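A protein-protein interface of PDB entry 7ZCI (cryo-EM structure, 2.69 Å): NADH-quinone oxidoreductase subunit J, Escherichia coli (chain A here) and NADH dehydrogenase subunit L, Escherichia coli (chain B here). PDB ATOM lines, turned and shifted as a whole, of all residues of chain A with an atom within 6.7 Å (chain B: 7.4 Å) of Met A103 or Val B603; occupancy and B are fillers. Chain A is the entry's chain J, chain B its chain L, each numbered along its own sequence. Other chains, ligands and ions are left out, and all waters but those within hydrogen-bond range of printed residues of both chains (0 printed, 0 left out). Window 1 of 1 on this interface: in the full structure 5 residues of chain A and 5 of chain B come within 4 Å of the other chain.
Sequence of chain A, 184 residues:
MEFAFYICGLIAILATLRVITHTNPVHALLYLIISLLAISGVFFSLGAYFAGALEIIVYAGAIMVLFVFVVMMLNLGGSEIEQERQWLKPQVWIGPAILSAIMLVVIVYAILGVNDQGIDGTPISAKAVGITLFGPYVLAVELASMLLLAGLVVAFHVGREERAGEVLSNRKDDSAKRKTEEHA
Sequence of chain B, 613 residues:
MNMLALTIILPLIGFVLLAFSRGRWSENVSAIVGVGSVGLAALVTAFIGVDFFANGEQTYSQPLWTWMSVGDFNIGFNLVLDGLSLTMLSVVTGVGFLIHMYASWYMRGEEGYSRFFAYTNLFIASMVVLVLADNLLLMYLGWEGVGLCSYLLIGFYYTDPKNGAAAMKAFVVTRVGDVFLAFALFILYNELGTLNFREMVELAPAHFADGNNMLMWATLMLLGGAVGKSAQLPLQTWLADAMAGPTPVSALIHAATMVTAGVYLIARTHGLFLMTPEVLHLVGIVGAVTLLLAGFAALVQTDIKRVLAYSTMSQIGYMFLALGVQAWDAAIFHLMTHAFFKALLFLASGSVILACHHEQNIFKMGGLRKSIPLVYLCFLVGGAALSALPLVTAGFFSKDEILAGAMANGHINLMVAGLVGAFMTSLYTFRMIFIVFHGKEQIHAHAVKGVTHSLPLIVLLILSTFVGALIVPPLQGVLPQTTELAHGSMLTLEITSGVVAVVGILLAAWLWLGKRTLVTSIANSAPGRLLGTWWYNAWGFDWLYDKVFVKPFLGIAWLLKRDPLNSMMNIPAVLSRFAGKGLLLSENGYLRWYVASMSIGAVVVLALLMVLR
Ser B599 touches Leu A99 (OG to CD2, 3.3 Å).
Leu A99 touches Ile B600.
Leu A99 touches Val B603.
CG2 of Ile A102 touches CG1 of Val B603, at 3.7 Å.
Ser B599 touches Met A103.
Met A103 touches Val B603 (CB to CG2, 3.7 Å).
Val A106 touches Leu B606 (CG1 to CB, 3.6 Å).
Ile A107 touches Leu B606.
Of chain B, only Ser B599 (3.8 Å) and Val B603 (3.7 Å) come within 4 Å of Met A103.
Of chain A, only Leu A99 (3.8 Å), Ile A102 (3.7 Å) and Met A103 (3.7 Å) come within 4 Å of Val B603.
Of the printed residues of chain B, Val A106 touches Leu B606 (3.6 Å).
Of the printed residues of chain B, Leu A99 touches Ser B599, Ile B600 and Val B603.
Printed residues of chain B within 4 Å of Ile A107: Leu B606.
Of the printed residues of chain A, Leu B606 touches Val A106 and Ile A107.
Of the printed residues of chain A, Ile B600 touches Leu A99.
Ala B602 touches none of the printed residues of chain A.
Ile A98 touches none of the printed residues of chain B.
The nearest residue of chain B that does not touch Met A103 is Ala B602 (4.04 Å).
The nearest residue of chain A that does not touch Val B603 is Val A106 (5.4 Å).
Hydrophobic or aromatic side chains of chain A within 4 Å of the printed part of chain B: Leu A99, Ile A102, Met A103, Val A106 and Ile A107.
Of the 13 printed residues of chain B, 4 touch a printed residue of chain A.
Printed residues of chain B that touch a printed residue of chain A: Ser B599, Ile B600, Val B603 and Leu B606.
Among the printed residues, no Asp or Glu carboxylate lies within 4 Å of a Lys or Arg side-chain nitrogen of the other chain.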
ATOM      1  N   ILE A  98     -17.179  -0.625 -14.368  1.00  0.00           N
ATOM      2  CA  ILE A  98     -18.230  -0.282 -15.325  1.00  0.00           C
ATOM      3  C   ILE A  98     -17.876   0.992 -16.082  1.00  0.00           C
ATOM      4  O   ILE A  98     -18.144   1.101 -17.283  1.00  0.00           O
ATOM      5  CB  ILE A  98     -19.613  -0.181 -14.645  1.00  0.00           C
ATOM      6  CG1 ILE A  98     -19.968  -1.465 -13.895  1.00  0.00           C
ATOM      7  CG2 ILE A  98     -20.709   0.124 -15.650  1.00  0.00           C
ATOM      8  CD1 ILE A  98     -20.833  -1.241 -12.675  1.00  0.00           C
ATOM      9  N   LEU A  99     -17.249   1.961 -15.409  1.00  0.00           N
ATOM     10  CA  LEU A  99     -16.856   3.195 -16.091  1.00  0.00           C
ATOM     11  C   LEU A  99     -15.831   2.928 -17.192  1.00  0.00           C
ATOM     12  O   LEU A  99     -15.970   3.420 -18.325  1.00  0.00           O
ATOM     13  CB  LEU A  99     -16.304   4.184 -15.071  1.00  0.00           C
ATOM     14  CG  LEU A  99     -15.881   5.551 -15.588  1.00  0.00           C
ATOM     15  CD1 LEU A  99     -17.104   6.367 -15.945  1.00  0.00           C
ATOM     16  CD2 LEU A  99     -15.060   6.252 -14.532  1.00  0.00           C
ATOM     17  N   SER A 100     -14.822   2.112 -16.890  1.00  0.00           N
ATOM     18  CA  SER A 100     -13.819   1.749 -17.878  1.00  0.00           C
ATOM     19  C   SER A 100     -14.392   0.860 -18.971  1.00  0.00           C
ATOM     20  O   SER A 100     -13.964   0.955 -20.123  1.00  0.00           O
ATOM     21  CB  SER A 100     -12.654   1.055 -17.188  1.00  0.00           C
ATOM     22  OG  SER A 100     -11.802   2.000 -16.569  1.00  0.00           O
ATOM     23  N   ALA A 101     -15.357   0.001 -18.639  1.00  0.00           N
ATOM     24  CA  ALA A 101     -16.016  -0.804 -19.660  1.00  0.00           C
ATOM     25  C   ALA A 101     -16.828   0.063 -20.612  1.00  0.00           C
ATOM     26  O   ALA A 101     -16.836  -0.187 -21.819  1.00  0.00           O
ATOM     27  CB  ALA A 101     -16.902  -1.860 -19.006  1.00  0.00           C
ATOM     28  N   ILE A 102     -17.517   1.084 -20.091  1.00  0.00           N
ATOM     29  CA  ILE A 102     -18.257   2.006 -20.951  1.00  0.00           C
ATOM     30  C   ILE A 102     -17.304   2.752 -21.873  1.00  0.00           C
ATOM     31  O   ILE A 102     -17.562   2.892 -23.077  1.00  0.00           O
ATOM     32  CB  ILE A 102     -19.102   2.983 -20.109  1.00  0.00           C
ATOM     33  CG1 ILE A 102     -20.265   2.261 -19.436  1.00  0.00           C
ATOM     34  CG2 ILE A 102     -19.645   4.108 -20.964  1.00  0.00           C
ATOM     35  CD1 ILE A 102     -20.718   2.928 -18.160  1.00  0.00           C
ATOM     36  N   MET A 103     -16.178   3.223 -21.326  1.00  0.00           N
ATOM     37  CA  MET A 103     -15.185   3.896 -22.159  1.00  0.00           C
ATOM     38  C   MET A 103     -14.613   2.951 -23.212  1.00  0.00           C
ATOM     39  O   MET A 103     -14.374   3.358 -24.356  1.00  0.00           O
ATOM     40  CB  MET A 103     -14.074   4.478 -21.291  1.00  0.00           C
ATOM     41  CG  MET A 103     -13.028   5.244 -22.073  1.00  0.00           C
ATOM     42  SD  MET A 103     -11.568   5.623 -21.102  1.00  0.00           S
ATOM     43  CE  MET A 103     -12.310   6.607 -19.811  1.00  0.00           C
ATOM     44  N   LEU A 104     -14.423   1.681 -22.852  1.00  0.00           N
ATOM     45  CA  LEU A 104     -13.929   0.696 -23.806  1.00  0.00           C
ATOM     46  C   LEU A 104     -14.922   0.453 -24.933  1.00  0.00           C
ATOM     47  O   LEU A 104     -14.524   0.378 -26.097  1.00  0.00           O
ATOM     48  CB  LEU A 104     -13.608  -0.612 -23.089  1.00  0.00           C
ATOM     49  CG  LEU A 104     -13.023  -1.718 -23.965  1.00  0.00           C
ATOM     50  CD1 LEU A 104     -11.715  -1.264 -24.574  1.00  0.00           C
ATOM     51  CD2 LEU A 104     -12.824  -2.980 -23.154  1.00  0.00           C
ATOM     52  N   VAL A 105     -16.215   0.331 -24.614  1.00  0.00           N
ATOM     53  CA  VAL A 105     -17.220   0.126 -25.658  1.00  0.00           C
ATOM     54  C   VAL A 105     -17.323   1.346 -26.565  1.00  0.00           C
ATOM     55  O   VAL A 105     -17.460   1.208 -27.786  1.00  0.00           O
ATOM     56  CB  VAL A 105     -18.588  -0.252 -25.058  1.00  0.00           C
ATOM     57  CG1 VAL A 105     -19.560  -0.615 -26.159  1.00  0.00           C
ATOM     58  CG2 VAL A 105     -18.453  -1.464 -24.182  1.00  0.00           C
ATOM     59  N   VAL A 106     -17.234   2.552 -26.000  1.00  0.00           N
ATOM     60  CA  VAL A 106     -17.304   3.757 -26.828  1.00  0.00           C
ATOM     61  C   VAL A 106     -16.100   3.841 -27.764  1.00  0.00           C
ATOM     62  O   VAL A 106     -16.246   4.088 -28.972  1.00  0.00           O
ATOM     63  CB  VAL A 106     -17.422   5.012 -25.947  1.00  0.00           C
ATOM     64  CG1 VAL A 106     -17.283   6.248 -26.791  1.00  0.00           C
ATOM     65  CG2 VAL A 106     -18.755   5.027 -25.233  1.00  0.00           C
ATOM     66  N   ILE A 107     -14.898   3.597 -27.230  1.00  0.00           N
ATOM     67  CA  ILE A 107     -13.693   3.657 -28.053  1.00  0.00           C
ATOM     68  C   ILE A 107     -13.718   2.574 -29.124  1.00  0.00           C
ATOM     69  O   ILE A 107     -13.414   2.838 -30.288  1.00  0.00           O
ATOM     70  CB  ILE A 107     -12.433   3.561 -27.172  1.00  0.00           C
ATOM     71  CG1 ILE A 107     -12.262   4.829 -26.343  1.00  0.00           C
ATOM     72  CG2 ILE A 107     -11.198   3.382 -28.026  1.00  0.00           C
ATOM     73  CD1 ILE A 107     -11.161   4.728 -25.312  1.00  0.00           C
ATOM     74  N   VAL A 108     -14.129   1.354 -28.762  1.00  0.00           N
ATOM     75  CA  VAL A 108     -14.153   0.246 -29.711  1.00  0.00           C
ATOM     76  C   VAL A 108     -15.196   0.485 -30.799  1.00  0.00           C
ATOM     77  O   VAL A 108     -14.967   0.166 -31.971  1.00  0.00           O
ATOM     78  CB  VAL A 108     -14.378  -1.078 -28.956  1.00  0.00           C
ATOM     79  CG1 VAL A 108     -14.921  -2.169 -29.864  1.00  0.00           C
ATOM     80  CG2 VAL A 108     -13.079  -1.537 -28.322  1.00  0.00           C
ATOM     81  N   SER B 597     -12.957  11.513 -11.724  1.00  0.00           N
ATOM     82  CA  SER B 597     -13.703  12.590 -12.364  1.00  0.00           C
ATOM     83  C   SER B 597     -13.185  12.859 -13.766  1.00  0.00           C
ATOM     84  O   SER B 597     -13.970  13.145 -14.677  1.00  0.00           O
ATOM     85  CB  SER B 597     -13.626  13.855 -11.518  1.00  0.00           C
ATOM     86  OG  SER B 597     -12.327  14.409 -11.556  1.00  0.00           O
ATOM     87  N   MET B 598     -11.867  12.771 -13.960  1.00  0.00           N
ATOM     88  CA  MET B 598     -11.314  12.904 -15.306  1.00  0.00           C
ATOM     89  C   MET B 598     -11.794  11.780 -16.218  1.00  0.00           C
ATOM     90  O   MET B 598     -12.125  12.018 -17.383  1.00  0.00           O
ATOM     91  CB  MET B 598      -9.789  12.935 -15.257  1.00  0.00           C
ATOM     92  CG  MET B 598      -9.213  14.261 -14.803  1.00  0.00           C
ATOM     93  SD  MET B 598      -7.671  14.682 -15.637  1.00  0.00           S
ATOM     94  CE  MET B 598      -6.887  13.081 -15.769  1.00  0.00           C
ATOM     95  N   SER B 599     -11.854  10.551 -15.702  1.00  0.00           N
ATOM     96  CA  SER B 599     -12.327   9.443 -16.529  1.00  0.00           C
ATOM     97  C   SER B 599     -13.825   9.544 -16.804  1.00  0.00           C
ATOM     98  O   SER B 599     -14.287   9.185 -17.896  1.00  0.00           O
ATOM     99  CB  SER B 599     -11.985   8.108 -15.872  1.00  0.00           C
ATOM    100  OG  SER B 599     -12.323   8.115 -14.502  1.00  0.00           O
ATOM    101  N   ILE B 600     -14.597  10.042 -15.832  1.00  0.00           N
ATOM    102  CA  ILE B 600     -16.026  10.274 -16.039  1.00  0.00           C
ATOM    103  C   ILE B 600     -16.240  11.336 -17.109  1.00  0.00           C
ATOM    104  O   ILE B 600     -17.092  11.184 -17.996  1.00  0.00           O
ATOM    105  CB  ILE B 600     -16.696  10.663 -14.705  1.00  0.00           C
ATOM    106  CG1 ILE B 600     -16.914   9.433 -13.830  1.00  0.00           C
ATOM    107  CG2 ILE B 600     -18.031  11.342 -14.932  1.00  0.00           C
ATOM    108  CD1 ILE B 600     -17.335   9.766 -12.421  1.00  0.00           C
ATOM    109  N   GLY B 601     -15.459  12.418 -17.054  1.00  0.00           N
ATOM    110  CA  GLY B 601     -15.550  13.444 -18.077  1.00  0.00           C
ATOM    111  C   GLY B 601     -15.128  12.944 -19.444  1.00  0.00           C
ATOM    112  O   GLY B 601     -15.693  13.349 -20.460  1.00  0.00           O
ATOM    113  N   ALA B 602     -14.134  12.055 -19.485  1.00  0.00           N
ATOM    114  CA  ALA B 602     -13.739  11.435 -20.745  1.00  0.00           C
ATOM    115  C   ALA B 602     -14.868  10.602 -21.329  1.00  0.00           C
ATOM    116  O   ALA B 602     -15.144  10.674 -22.533  1.00  0.00           O
ATOM    117  CB  ALA B 602     -12.498  10.572 -20.537  1.00  0.00           C
ATOM    118  N   VAL B 603     -15.542   9.819 -20.483  1.00  0.00           N
ATOM    119  CA  VAL B 603     -16.675   9.014 -20.931  1.00  0.00           C
ATOM    120  C   VAL B 603     -17.791   9.908 -21.455  1.00  0.00           C
ATOM    121  O   VAL B 603     -18.376   9.642 -22.512  1.00  0.00           O
ATOM    122  CB  VAL B 603     -17.159   8.105 -19.786  1.00  0.00           C
ATOM    123  CG1 VAL B 603     -18.546   7.557 -20.068  1.00  0.00           C
ATOM    124  CG2 VAL B 603     -16.181   6.974 -19.559  1.00  0.00           C
ATOM    125  N   VAL B 604     -18.075  11.000 -20.740  1.00  0.00           N
ATOM    126  CA  VAL B 604     -19.144  11.915 -21.133  1.00  0.00           C
ATOM    127  C   VAL B 604     -18.822  12.598 -22.459  1.00  0.00           C
ATOM    128  O   VAL B 604     -19.678  12.681 -23.348  1.00  0.00           O
ATOM    129  CB  VAL B 604     -19.395  12.934 -20.006  1.00  0.00           C
ATOM    130  CG1 VAL B 604     -20.217  14.105 -20.503  1.00  0.00           C
ATOM    131  CG2 VAL B 604     -20.096  12.262 -18.844  1.00  0.00           C
ATOM    132  N   VAL B 605     -17.584  13.076 -22.625  1.00  0.00           N
ATOM    133  CA  VAL B 605     -17.191  13.759 -23.856  1.00  0.00           C
ATOM    134  C   VAL B 605     -17.228  12.802 -25.043  1.00  0.00           C
ATOM    135  O   VAL B 605     -17.736  13.147 -26.119  1.00  0.00           O
ATOM    136  CB  VAL B 605     -15.802  14.403 -23.681  1.00  0.00           C
ATOM    137  CG1 VAL B 605     -15.191  14.768 -25.020  1.00  0.00           C
ATOM    138  CG2 VAL B 605     -15.897  15.629 -22.805  1.00  0.00           C
ATOM    139  N   LEU B 606     -16.717  11.581 -24.862  1.00  0.00           N
ATOM    140  CA  LEU B 606     -16.736  10.605 -25.945  1.00  0.00           C
ATOM    141  C   LEU B 606     -18.158  10.202 -26.316  1.00  0.00           C
ATOM    142  O   LEU B 606     -18.482  10.089 -27.503  1.00  0.00           O
ATOM    143  CB  LEU B 606     -15.914   9.382 -25.557  1.00  0.00           C
ATOM    144  CG  LEU B 606     -14.397   9.542 -25.549  1.00  0.00           C
ATOM    145  CD1 LEU B 606     -13.750   8.229 -25.166  1.00  0.00           C
ATOM    146  CD2 LEU B 606     -13.900  10.016 -26.895  1.00  0.00           C
ATOM    147  N   ALA B 607     -19.026   9.999 -25.320  1.00  0.00           N
ATOM    148  CA  ALA B 607     -20.410   9.639 -25.603  1.00  0.00           C
ATOM    149  C   ALA B 607     -21.149  10.774 -26.296  1.00  0.00           C
ATOM    150  O   ALA B 607     -21.979  10.531 -27.179  1.00  0.00           O
ATOM    151  CB  ALA B 607     -21.124   9.247 -24.312  1.00  0.00           C
ATOM    152  N   LEU B 608     -20.864  12.020 -25.906  1.00  0.00           N
ATOM    153  CA  LEU B 608     -21.471  13.169 -26.568  1.00  0.00           C
ATOM    154  C   LEU B 608     -21.016  13.280 -28.015  1.00  0.00           C
ATOM    155  O   LEU B 608     -21.817  13.603 -28.897  1.00  0.00           O
ATOM    156  CB  LEU B 608     -21.136  14.446 -25.805  1.00  0.00           C
ATOM    157  CG  LEU B 608     -22.009  14.780 -24.599  1.00  0.00           C
ATOM    158  CD1 LEU B 608     -21.461  15.993 -23.875  1.00  0.00           C
ATOM    159  CD2 LEU B 608     -23.436  15.022 -25.032  1.00  0.00           C
ATOM    160  N   LEU B 609     -19.736  13.014 -28.279  1.00  0.00           N
ATOM    161  CA  LEU B 609     -19.246  13.069 -29.653  1.00  0.00           C
ATOM    162  C   LEU B 609     -19.832  11.946 -30.500  1.00  0.00           C
ATOM    163  O   LEU B 609     -20.090  12.136 -31.692  1.00  0.00           O
ATOM    164  CB  LEU B 609     -17.723  13.014 -29.670  1.00  0.00           C
ATOM    165  CG  LEU B 609     -17.049  14.349 -29.380  1.00  0.00           C
ATOM    166  CD1 LEU B 609     -15.594  14.138 -29.086  1.00  0.00           C
ATOM    167  CD2 LEU B 609     -17.214  15.288 -30.544  1.00  0.00           C
